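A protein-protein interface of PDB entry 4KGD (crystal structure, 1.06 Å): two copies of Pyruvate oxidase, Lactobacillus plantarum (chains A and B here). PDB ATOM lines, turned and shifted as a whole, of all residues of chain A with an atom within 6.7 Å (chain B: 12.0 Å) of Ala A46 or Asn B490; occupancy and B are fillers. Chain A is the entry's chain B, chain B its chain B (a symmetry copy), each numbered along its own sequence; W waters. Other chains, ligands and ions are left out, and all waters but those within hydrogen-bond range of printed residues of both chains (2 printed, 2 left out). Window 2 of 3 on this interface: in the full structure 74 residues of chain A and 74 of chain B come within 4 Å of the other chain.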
ATOM      1  N   LEU A  12      -3.869   1.580  33.323  1.00  0.00           N
ATOM      2  CA  LEU A  12      -4.199   3.005  33.176  1.00  0.00           C
ATOM      3  C   LEU A  12      -5.569   3.264  33.734  1.00  0.00           C
ATOM      4  O   LEU A  12      -6.525   2.474  33.528  1.00  0.00           O
ATOM      5  CB  LEU A  12      -4.174   3.386  31.709  1.00  0.00           C
ATOM      6  CG  LEU A  12      -2.814   3.404  31.054  1.00  0.00           C
ATOM      7  CD1 LEU A  12      -2.931   3.629  29.558  1.00  0.00           C
ATOM      8  CD2 LEU A  12      -1.932   4.494  31.655  1.00  0.00           C
ATOM      9  N   MET A  41     -10.622   8.793  25.014  1.00  0.00           N
ATOM     10  CA  MET A  41     -10.616   8.269  23.665  1.00  0.00           C
ATOM     11  C   MET A  41      -9.576   7.175  23.494  1.00  0.00           C
ATOM     12  O   MET A  41      -9.828   6.147  22.854  1.00  0.00           O
ATOM     13  CB  MET A  41     -10.355   9.342  22.593  1.00  0.00           C
ATOM     14  CG  MET A  41     -11.362  10.498  22.515  1.00  0.00           C
ATOM     15  SD  MET A  41     -13.062  10.015  22.428  1.00  0.00           S
ATOM     16  CE  MET A  41     -13.079   9.035  20.967  1.00  0.00           C
ATOM     17  N   ASP A  42      -8.399   7.387  24.068  1.00  0.00           N
ATOM     18  CA  ASP A  42      -7.294   6.429  23.919  1.00  0.00           C
ATOM     19  C   ASP A  42      -7.703   5.095  24.515  1.00  0.00           C
ATOM     20  O   ASP A  42      -7.397   4.041  23.957  1.00  0.00           O
ATOM     21  CB  ASP A  42      -6.039   7.019  24.571  1.00  0.00           C
ATOM     22  CG  ASP A  42      -4.743   6.576  23.965  1.00  0.00           C
ATOM     23  OD1 ASP A  42      -4.732   6.009  22.840  1.00  0.00           O
ATOM     24  OD2 ASP A  42      -3.690   6.820  24.612  1.00  0.00           O
ATOM     25  N   ALA A  43      -8.390   5.127  25.653  1.00  0.00           N
ATOM     26  CA  ALA A  43      -8.864   3.899  26.286  1.00  0.00           C
ATOM     27  C   ALA A  43      -9.940   3.192  25.483  1.00  0.00           C
ATOM     28  O   ALA A  43      -9.926   1.963  25.321  1.00  0.00           O
ATOM     29  CB  ALA A  43      -9.326   4.187  27.690  1.00  0.00           C
ATOM     30  N   LEU A  44     -10.847   3.962  24.898  1.00  0.00           N
ATOM     31  CA  LEU A  44     -11.848   3.409  24.020  1.00  0.00           C
ATOM     32  C   LEU A  44     -11.240   2.713  22.802  1.00  0.00           C
ATOM     33  O   LEU A  44     -11.686   1.690  22.313  1.00  0.00           O
ATOM     34  CB  LEU A  44     -12.847   4.464  23.527  1.00  0.00           C
ATOM     35  CG  LEU A  44     -13.820   4.975  24.557  1.00  0.00           C
ATOM     36  CD1 LEU A  44     -14.528   6.241  24.022  1.00  0.00           C
ATOM     37  CD2 LEU A  44     -14.808   3.895  24.910  1.00  0.00           C
ATOM     38  N   SER A  45     -10.165   3.333  22.290  1.00  0.00           N
ATOM     39  CA  SER A  45      -9.545   2.855  21.072  1.00  0.00           C
ATOM     40  C   SER A  45      -8.981   1.443  21.249  1.00  0.00           C
ATOM     41  O   SER A  45      -8.967   0.668  20.276  1.00  0.00           O
ATOM     42  CB  SER A  45      -8.448   3.834  20.707  1.00  0.00           C
ATOM     43  OG  SER A  45      -7.860   3.411  19.512  1.00  0.00           O
ATOM     44  N   ALA A  46      -8.509   1.114  22.446  1.00  0.00           N
ATOM     45  CA  ALA A  46      -8.008  -0.225  22.721  1.00  0.00           C
ATOM     46  C   ALA A  46      -9.077  -1.263  22.977  1.00  0.00           C
ATOM     47  O   ALA A  46      -8.767  -2.444  23.059  1.00  0.00           O
ATOM     48  CB  ALA A  46      -7.072  -0.135  23.920  1.00  0.00           C
ATOM     49  N   GLU A  47     -10.347  -0.858  23.133  1.00  0.00           N
ATOM     50  CA  GLU A  47     -11.462  -1.684  23.524  1.00  0.00           C
ATOM     51  C   GLU A  47     -12.592  -1.750  22.495  1.00  0.00           C
ATOM     52  O   GLU A  47     -13.736  -1.987  22.818  1.00  0.00           O
ATOM     53  CB  GLU A  47     -12.001  -1.203  24.881  1.00  0.00           C
ATOM     54  CG  GLU A  47     -11.134  -1.476  26.074  1.00  0.00           C
ATOM     55  CD  GLU A  47     -11.060  -2.943  26.390  1.00  0.00           C
ATOM     56  OE1 GLU A  47     -12.094  -3.627  26.539  1.00  0.00           O
ATOM     57  OE2 GLU A  47      -9.928  -3.446  26.460  1.00  0.00           O
ATOM     58  N   ARG A  48     -12.253  -1.656  21.204  1.00  0.00           N
ATOM     59  CA  ARG A  48     -13.260  -1.716  20.182  1.00  0.00           C
ATOM     60  C   ARG A  48     -13.977  -3.034  20.053  1.00  0.00           C
ATOM     61  O   ARG A  48     -15.120  -3.011  19.559  1.00  0.00           O
ATOM     62  CB  ARG A  48     -12.591  -1.386  18.823  1.00  0.00           C
ATOM     63  CG  ARG A  48     -12.089   0.077  18.785  1.00  0.00           C
ATOM     64  CD  ARG A  48     -11.314   0.253  17.483  1.00  0.00           C
ATOM     65  NE  ARG A  48     -10.572   1.492  17.559  1.00  0.00           N
ATOM     66  CZ  ARG A  48     -10.588   2.496  16.678  1.00  0.00           C
ATOM     67  NH1 ARG A  48     -11.657   2.722  15.930  1.00  0.00           N
ATOM     68  NH2 ARG A  48      -9.657   3.376  16.565  1.00  0.00           N
ATOM     69  N   ASP A  49     -13.416  -4.148  20.469  1.00  0.00           N
ATOM     70  CA  ASP A  49     -14.165  -5.388  20.384  1.00  0.00           C
ATOM     71  C   ASP A  49     -15.290  -5.430  21.385  1.00  0.00           C
ATOM     72  O   ASP A  49     -16.264  -6.078  21.099  1.00  0.00           O
ATOM     73  CB  ASP A  49     -13.206  -6.577  20.579  1.00  0.00           C
ATOM     74  CG  ASP A  49     -13.968  -7.898  20.407  1.00  0.00           C
ATOM     75  OD1 ASP A  49     -13.895  -8.708  21.344  1.00  0.00           O
ATOM     76  OD2 ASP A  49     -14.621  -8.040  19.345  1.00  0.00           O
ATOM     77  N   ILE B 480      -7.915  17.684  15.827  1.00  0.00           N
ATOM     78  CA  ILE B 480      -7.908  16.666  16.885  1.00  0.00           C
ATOM     79  C   ILE B 480      -7.123  15.440  16.464  1.00  0.00           C
ATOM     80  O   ILE B 480      -6.464  14.823  17.314  1.00  0.00           O
ATOM     81  CB  ILE B 480      -9.327  16.270  17.299  1.00  0.00           C
ATOM     82  CG1 ILE B 480     -10.137  17.510  17.629  1.00  0.00           C
ATOM     83  CG2 ILE B 480      -9.306  15.289  18.455  1.00  0.00           C
ATOM     84  CD1 ILE B 480      -9.492  18.443  18.588  1.00  0.00           C
ATOM     85  N   LYS B 481      -7.196  15.047  15.214  1.00  0.00           N
ATOM     86  CA  LYS B 481      -6.372  13.955  14.697  1.00  0.00           C
ATOM     87  C   LYS B 481      -4.901  14.193  15.017  1.00  0.00           C
ATOM     88  O   LYS B 481      -4.180  13.328  15.535  1.00  0.00           O
ATOM     89  CB  LYS B 481      -6.600  13.764  13.223  1.00  0.00           C
ATOM     90  CG  LYS B 481      -5.750  12.670  12.622  1.00  0.00           C
ATOM     91  CD  LYS B 481      -6.048  12.423  11.176  1.00  0.00           C
ATOM     92  CE  LYS B 481      -5.157  11.366  10.536  1.00  0.00           C
ATOM     93  NZ  LYS B 481      -3.801  11.969  10.302  1.00  0.00           N
ATOM     94  N   ASP B 482      -4.443  15.427  14.755  1.00  0.00           N
ATOM     95  CA  ASP B 482      -3.062  15.753  15.000  1.00  0.00           C
ATOM     96  C   ASP B 482      -2.705  15.705  16.484  1.00  0.00           C
ATOM     97  O   ASP B 482      -1.624  15.299  16.869  1.00  0.00           O
ATOM     98  CB  ASP B 482      -2.763  17.111  14.348  1.00  0.00           C
ATOM     99  CG  ASP B 482      -2.834  17.047  12.848  1.00  0.00           C
ATOM    100  OD1 ASP B 482      -2.696  15.980  12.199  1.00  0.00           O
ATOM    101  OD2 ASP B 482      -3.031  18.147  12.257  1.00  0.00           O
ATOM    102  N   GLU B 483      -3.653  16.119  17.325  1.00  0.00           N
ATOM    103  CA  GLU B 483      -3.470  15.968  18.747  1.00  0.00           C
ATOM    104  C   GLU B 483      -3.299  14.508  19.149  1.00  0.00           C
ATOM    105  O   GLU B 483      -2.417  14.154  19.920  1.00  0.00           O
ATOM    106  CB  GLU B 483      -4.644  16.593  19.540  1.00  0.00           C
ATOM    107  CG  GLU B 483      -4.697  18.116  19.419  1.00  0.00           C
ATOM    108  CD  GLU B 483      -5.952  18.700  19.931  1.00  0.00           C
ATOM    109  OE1 GLU B 483      -6.808  18.018  20.541  1.00  0.00           O
ATOM    110  OE2 GLU B 483      -6.225  19.885  19.600  1.00  0.00           O
ATOM    111  N   GLN B 484      -4.197  13.642  18.651  1.00  0.00           N
ATOM    112  CA  GLN B 484      -4.068  12.208  18.939  1.00  0.00           C
ATOM    113  C   GLN B 484      -2.728  11.659  18.434  1.00  0.00           C
ATOM    114  O   GLN B 484      -2.126  10.810  19.100  1.00  0.00           O
ATOM    115  CB  GLN B 484      -5.220  11.396  18.320  1.00  0.00           C
ATOM    116  CG  GLN B 484      -6.556  11.704  18.963  1.00  0.00           C
ATOM    117  CD  GLN B 484      -7.686  10.818  18.500  1.00  0.00           C
ATOM    118  OE1 GLN B 484      -7.531   9.997  17.569  1.00  0.00           O
ATOM    119  NE2 GLN B 484      -8.823  10.948  19.138  1.00  0.00           N
ATOM    120  N   GLU B 485      -2.266  12.149  17.291  1.00  0.00           N
ATOM    121  CA  GLU B 485      -0.950  11.701  16.810  1.00  0.00           C
ATOM    122  C   GLU B 485       0.110  11.987  17.851  1.00  0.00           C
ATOM    123  O   GLU B 485       1.029  11.193  18.074  1.00  0.00           O
ATOM    124  CB  GLU B 485      -0.653  12.370  15.470  1.00  0.00           C
ATOM    125  CG  GLU B 485       0.692  11.913  14.878  1.00  0.00           C
ATOM    126  CD  GLU B 485       1.001  12.637  13.620  1.00  0.00           C
ATOM    127  OE1 GLU B 485       0.343  12.336  12.574  1.00  0.00           O
ATOM    128  OE2 GLU B 485       1.896  13.506  13.632  1.00  0.00           O
ATOM    129  N   ASP B 486       0.014  13.163  18.460  1.00  0.00           N
ATOM    130  CA  ASP B 486       0.994  13.639  19.408  1.00  0.00           C
ATOM    131  C   ASP B 486       0.894  12.967  20.748  1.00  0.00           C
ATOM    132  O   ASP B 486       1.942  12.737  21.401  1.00  0.00           O
ATOM    133  CB  ASP B 486       0.826  15.182  19.554  1.00  0.00           C
ATOM    134  CG  ASP B 486       1.250  15.961  18.367  1.00  0.00           C
ATOM    135  OD1 ASP B 486       1.886  15.413  17.438  1.00  0.00           O
ATOM    136  OD2 ASP B 486       0.894  17.155  18.309  1.00  0.00           O
ATOM    137  N   THR B 487      -0.318  12.630  21.244  1.00  0.00           N
ATOM    138  CA  THR B 487      -0.466  12.164  22.608  1.00  0.00           C
ATOM    139  C   THR B 487      -0.910  10.720  22.772  1.00  0.00           C
ATOM    140  O   THR B 487      -0.660  10.160  23.848  1.00  0.00           O
ATOM    141  CB  THR B 487      -1.492  13.017  23.379  1.00  0.00           C
ATOM    142  OG1 THR B 487      -2.762  12.949  22.706  1.00  0.00           O
ATOM    143  CG2 THR B 487      -1.080  14.481  23.442  1.00  0.00           C
ATOM    144  N   ASN B 488      -1.662  10.178  21.857  1.00  0.00           N
ATOM    145  CA  ASN B 488      -2.391   8.943  22.136  1.00  0.00           C
ATOM    146  C   ASN B 488      -1.535   7.755  21.790  1.00  0.00           C
ATOM    147  O   ASN B 488      -0.808   7.752  20.798  1.00  0.00           O
ATOM    148  CB  ASN B 488      -3.689   8.914  21.306  1.00  0.00           C
ATOM    149  CG  ASN B 488      -4.752   9.790  21.942  1.00  0.00           C
ATOM    150  OD1 ASN B 488      -4.494  10.816  22.545  1.00  0.00           O
ATOM    151  ND2 ASN B 488      -6.011   9.373  21.772  1.00  0.00           N
ATOM    152  N   GLN B 489      -1.644   6.701  22.604  1.00  0.00           N
ATOM    153  CA  GLN B 489      -0.940   5.461  22.465  1.00  0.00           C
ATOM    154  C   GLN B 489      -1.564   4.530  21.436  1.00  0.00           C
ATOM    155  O   GLN B 489      -0.853   3.798  20.751  1.00  0.00           O
ATOM    156  CB  GLN B 489      -0.957   4.686  23.803  1.00  0.00           C
ATOM    157  CG  GLN B 489      -0.333   3.298  23.645  1.00  0.00           C
ATOM    158  CD  GLN B 489      -0.342   2.539  24.961  1.00  0.00           C
ATOM    159  OE1 GLN B 489      -1.253   2.750  25.812  1.00  0.00           O
ATOM    160  NE2 GLN B 489       0.690   1.712  25.034  1.00  0.00           N
ATOM    161  N   ASN B 490      -2.857   4.559  21.387  1.00  0.00           N
ATOM    162  CA  ASN B 490      -3.644   3.651  20.558  1.00  0.00           C
ATOM    163  C   ASN B 490      -4.078   4.332  19.267  1.00  0.00           C
ATOM    164  O   ASN B 490      -3.765   5.496  19.008  1.00  0.00           O
ATOM    165  CB  ASN B 490      -4.803   3.081  21.370  1.00  0.00           C
ATOM    166  CG  ASN B 490      -4.303   2.389  22.627  1.00  0.00           C
ATOM    167  OD1 ASN B 490      -3.383   1.562  22.522  1.00  0.00           O
ATOM    168  ND2 ASN B 490      -4.818   2.709  23.770  1.00  0.00           N
ATOM    169  N   ASP B 491      -4.784   3.616  18.394  1.00  0.00           N
ATOM    170  CA  ASP B 491      -5.075   4.097  17.069  1.00  0.00           C
ATOM    171  C   ASP B 491      -6.003   5.330  17.126  1.00  0.00           C
ATOM    172  O   ASP B 491      -6.757   5.522  18.078  1.00  0.00           O
ATOM    173  CB  ASP B 491      -5.751   2.989  16.267  1.00  0.00           C
ATOM    174  CG  ASP B 491      -4.935   1.760  15.990  1.00  0.00           C
ATOM    175  OD1 ASP B 491      -3.745   1.735  16.390  1.00  0.00           O
ATOM    176  OD2 ASP B 491      -5.433   0.765  15.378  1.00  0.00           O
ATOM    177  N   PHE B 492      -5.943   6.118  16.060  1.00  0.00           N
ATOM    178  CA  PHE B 492      -6.863   7.247  15.904  1.00  0.00           C
ATOM    179  C   PHE B 492      -8.306   6.749  16.127  1.00  0.00           C
ATOM    180  O   PHE B 492      -8.700   5.666  15.702  1.00  0.00           O
ATOM    181  CB  PHE B 492      -6.777   7.779  14.493  1.00  0.00           C
ATOM    182  CG  PHE B 492      -5.485   8.485  14.133  1.00  0.00           C
ATOM    183  CD1 PHE B 492      -5.028   9.536  14.888  1.00  0.00           C
ATOM    184  CD2 PHE B 492      -4.744   8.110  13.018  1.00  0.00           C
ATOM    185  CE1 PHE B 492      -3.884  10.199  14.549  1.00  0.00           C
ATOM    186  CE2 PHE B 492      -3.552   8.748  12.671  1.00  0.00           C
ATOM    187  CZ  PHE B 492      -3.144   9.786  13.447  1.00  0.00           C
ATOM    188  N   ILE B 493      -9.086   7.633  16.768  1.00  0.00           N
ATOM    189  CA  ILE B 493     -10.500   7.268  17.024  1.00  0.00           C
ATOM    190  C   ILE B 493     -11.332   8.529  16.997  1.00  0.00           C
ATOM    191  O   ILE B 493     -11.018   9.539  17.643  1.00  0.00           O
ATOM    192  CB  ILE B 493     -10.617   6.507  18.344  1.00  0.00           C
ATOM    193  CG1 ILE B 493     -12.066   6.080  18.590  1.00  0.00           C
ATOM    194  CG2 ILE B 493     -10.013   7.226  19.511  1.00  0.00           C
ATOM    195  CD1 ILE B 493     -12.227   5.026  19.679  1.00  0.00           C
ATOM    196  N   GLY B 494     -12.454   8.459  16.282  1.00  0.00           N
ATOM    197  CA  GLY B 494     -13.381   9.545  16.200  1.00  0.00           C
ATOM    198  C   GLY B 494     -12.965  10.721  15.368  1.00  0.00           C
ATOM    199  O   GLY B 494     -13.695  11.731  15.370  1.00  0.00           O
ATOM    200  N   VAL B 495     -11.845  10.641  14.647  1.00  0.00           N
ATOM    201  CA  VAL B 495     -11.277  11.785  13.956  1.00  0.00           C
ATOM    202  C   VAL B 495     -11.276  11.683  12.461  1.00  0.00           C
ATOM    203  O   VAL B 495     -10.975  12.694  11.801  1.00  0.00           O
ATOM    204  CB  VAL B 495      -9.848  12.120  14.477  1.00  0.00           C
ATOM    205  CG1 VAL B 495      -9.893  12.556  15.942  1.00  0.00           C
ATOM    206  CG2 VAL B 495      -8.897  10.969  14.237  1.00  0.00           C
ATOM    207  N   GLU B 496     -11.589  10.510  11.912  1.00  0.00           N
ATOM    208  CA  GLU B 496     -11.750  10.312  10.471  1.00  0.00           C
ATOM    209  C   GLU B 496     -13.164   9.804  10.214  1.00  0.00           C
ATOM    210  O   GLU B 496     -13.603   8.862  10.895  1.00  0.00           O
ATOM    211  CB  GLU B 496     -10.718   9.339   9.926  1.00  0.00           C
ATOM    212  CG  GLU B 496      -9.279   9.814  10.255  1.00  0.00           C
ATOM    213  CD  GLU B 496      -8.241   9.134   9.473  1.00  0.00           C
ATOM    214  OE1 GLU B 496      -7.772   9.535   8.366  1.00  0.00           O
ATOM    215  OE2 GLU B 496      -7.763   8.119   9.861  1.00  0.00           O
HETATM  216  O   HOH W   1      -2.865   5.027  26.566  1.00  0.00           O
HETATM  217  O   HOH W   2      -6.174   1.063  19.010  1.00  0.00           O
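The backbone carbonyl oxygen (O) of Phe B492 sits at hydrogen-bond distance from the guanidinium group (NH2) of Arg A48, at 2.6 Å.
N of Asn B490 lies within hydrogen-bond range of OD1 of Asp A42 (2.8 Å).
OG of Ser A45 is in hydrogen-bond range of O of Asp B491, 2.8 Å away.
The backbone NH of Gln B489 is in hydrogen-bond range of the side-chain carboxylate of Asp A42.
The backbone carbonyl oxygen (O) of Ser A45 is in hydrogen-bond range of the guanidinium group (NE) of Arg A48, at 3.3 Å.
The side-chain hydroxyl (OG1) of Thr B487 lies within hydrogen-bond range of the side-chain amide oxygen (OD1) of Asn B488, at 2.8 Å.
N of Ile B493 sits at hydrogen-bond distance from OE1 of Gln B484.
Among the printed residues, merely in contact across the chains: Met A41 with Ile B493, Asp A42 with Asn B488, Leu A44 with Ile B493, Ser A45 with Asn B490, Ser A45 with Ile B493, Ala A46 with Asn B490, Arg A48 with Asp B491 and Arg A48 with Ile B493.
No residue of chain B comes within 4 Å of Ala A43.
Of the printed residues of chain B, Leu A44 touches Ile B493.
Of chain B, only Asn B490 (3.6 Å), Asp B491 (2.8 Å) and Ile B493 (3.7 Å) come within 4 Å of Ser A45.
Of the printed residues of chain B, Ala A46 touches Asn B490 (3.6 Å).
Arg A48 touches just these residues of chain B: Asp B491, Phe B492 and Ile B493.
Asp B482 touches none of the printed residues of chain A.
Of the printed residues of chain A, Asn B490 touches Asp A42 (2.8 Å), Ser A45 (3.6 Å) and Ala A46 (3.6 Å).
Of the printed residues of chain A, Phe B492 touches Arg A48 (2.6 Å).
The nearest residue of chain A that does not touch Asn B490 is Ala A43 (4.7 Å).
The nearest printed residue of chain A that does not touch Ile B493 is Asp A42 (4.8 Å).
Hydrophobic or aromatic side chains of chain B within 4 Å of the printed part of chain A: Ile B493.
Printed residues of chain A that touch a printed residue of chain B: Met A41, Asp A42, Leu A44, Ser A45, Ala A46 and Arg A48.
Hydrophobic or aromatic side chains of chain A that line the printed part of chain B: Met A41, Leu A44 and Ala A46.
Among the printed residues, 12 pairs touch across the chains.
No position is printed for both chains.
Of the 12 pairs that touch across the chains among the printed residues, none has its exchanged pair printed and touching as well.
Water W1 lies within hydrogen-bond range of the side-chain carboxylate (OD2) of Asp A42 (2.8 Å) and the side-chain amide oxygen (OE1) of Gln B489 (2.9 Å).
Water W2 bridges OG of Ser A45 and N of Asp B491.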
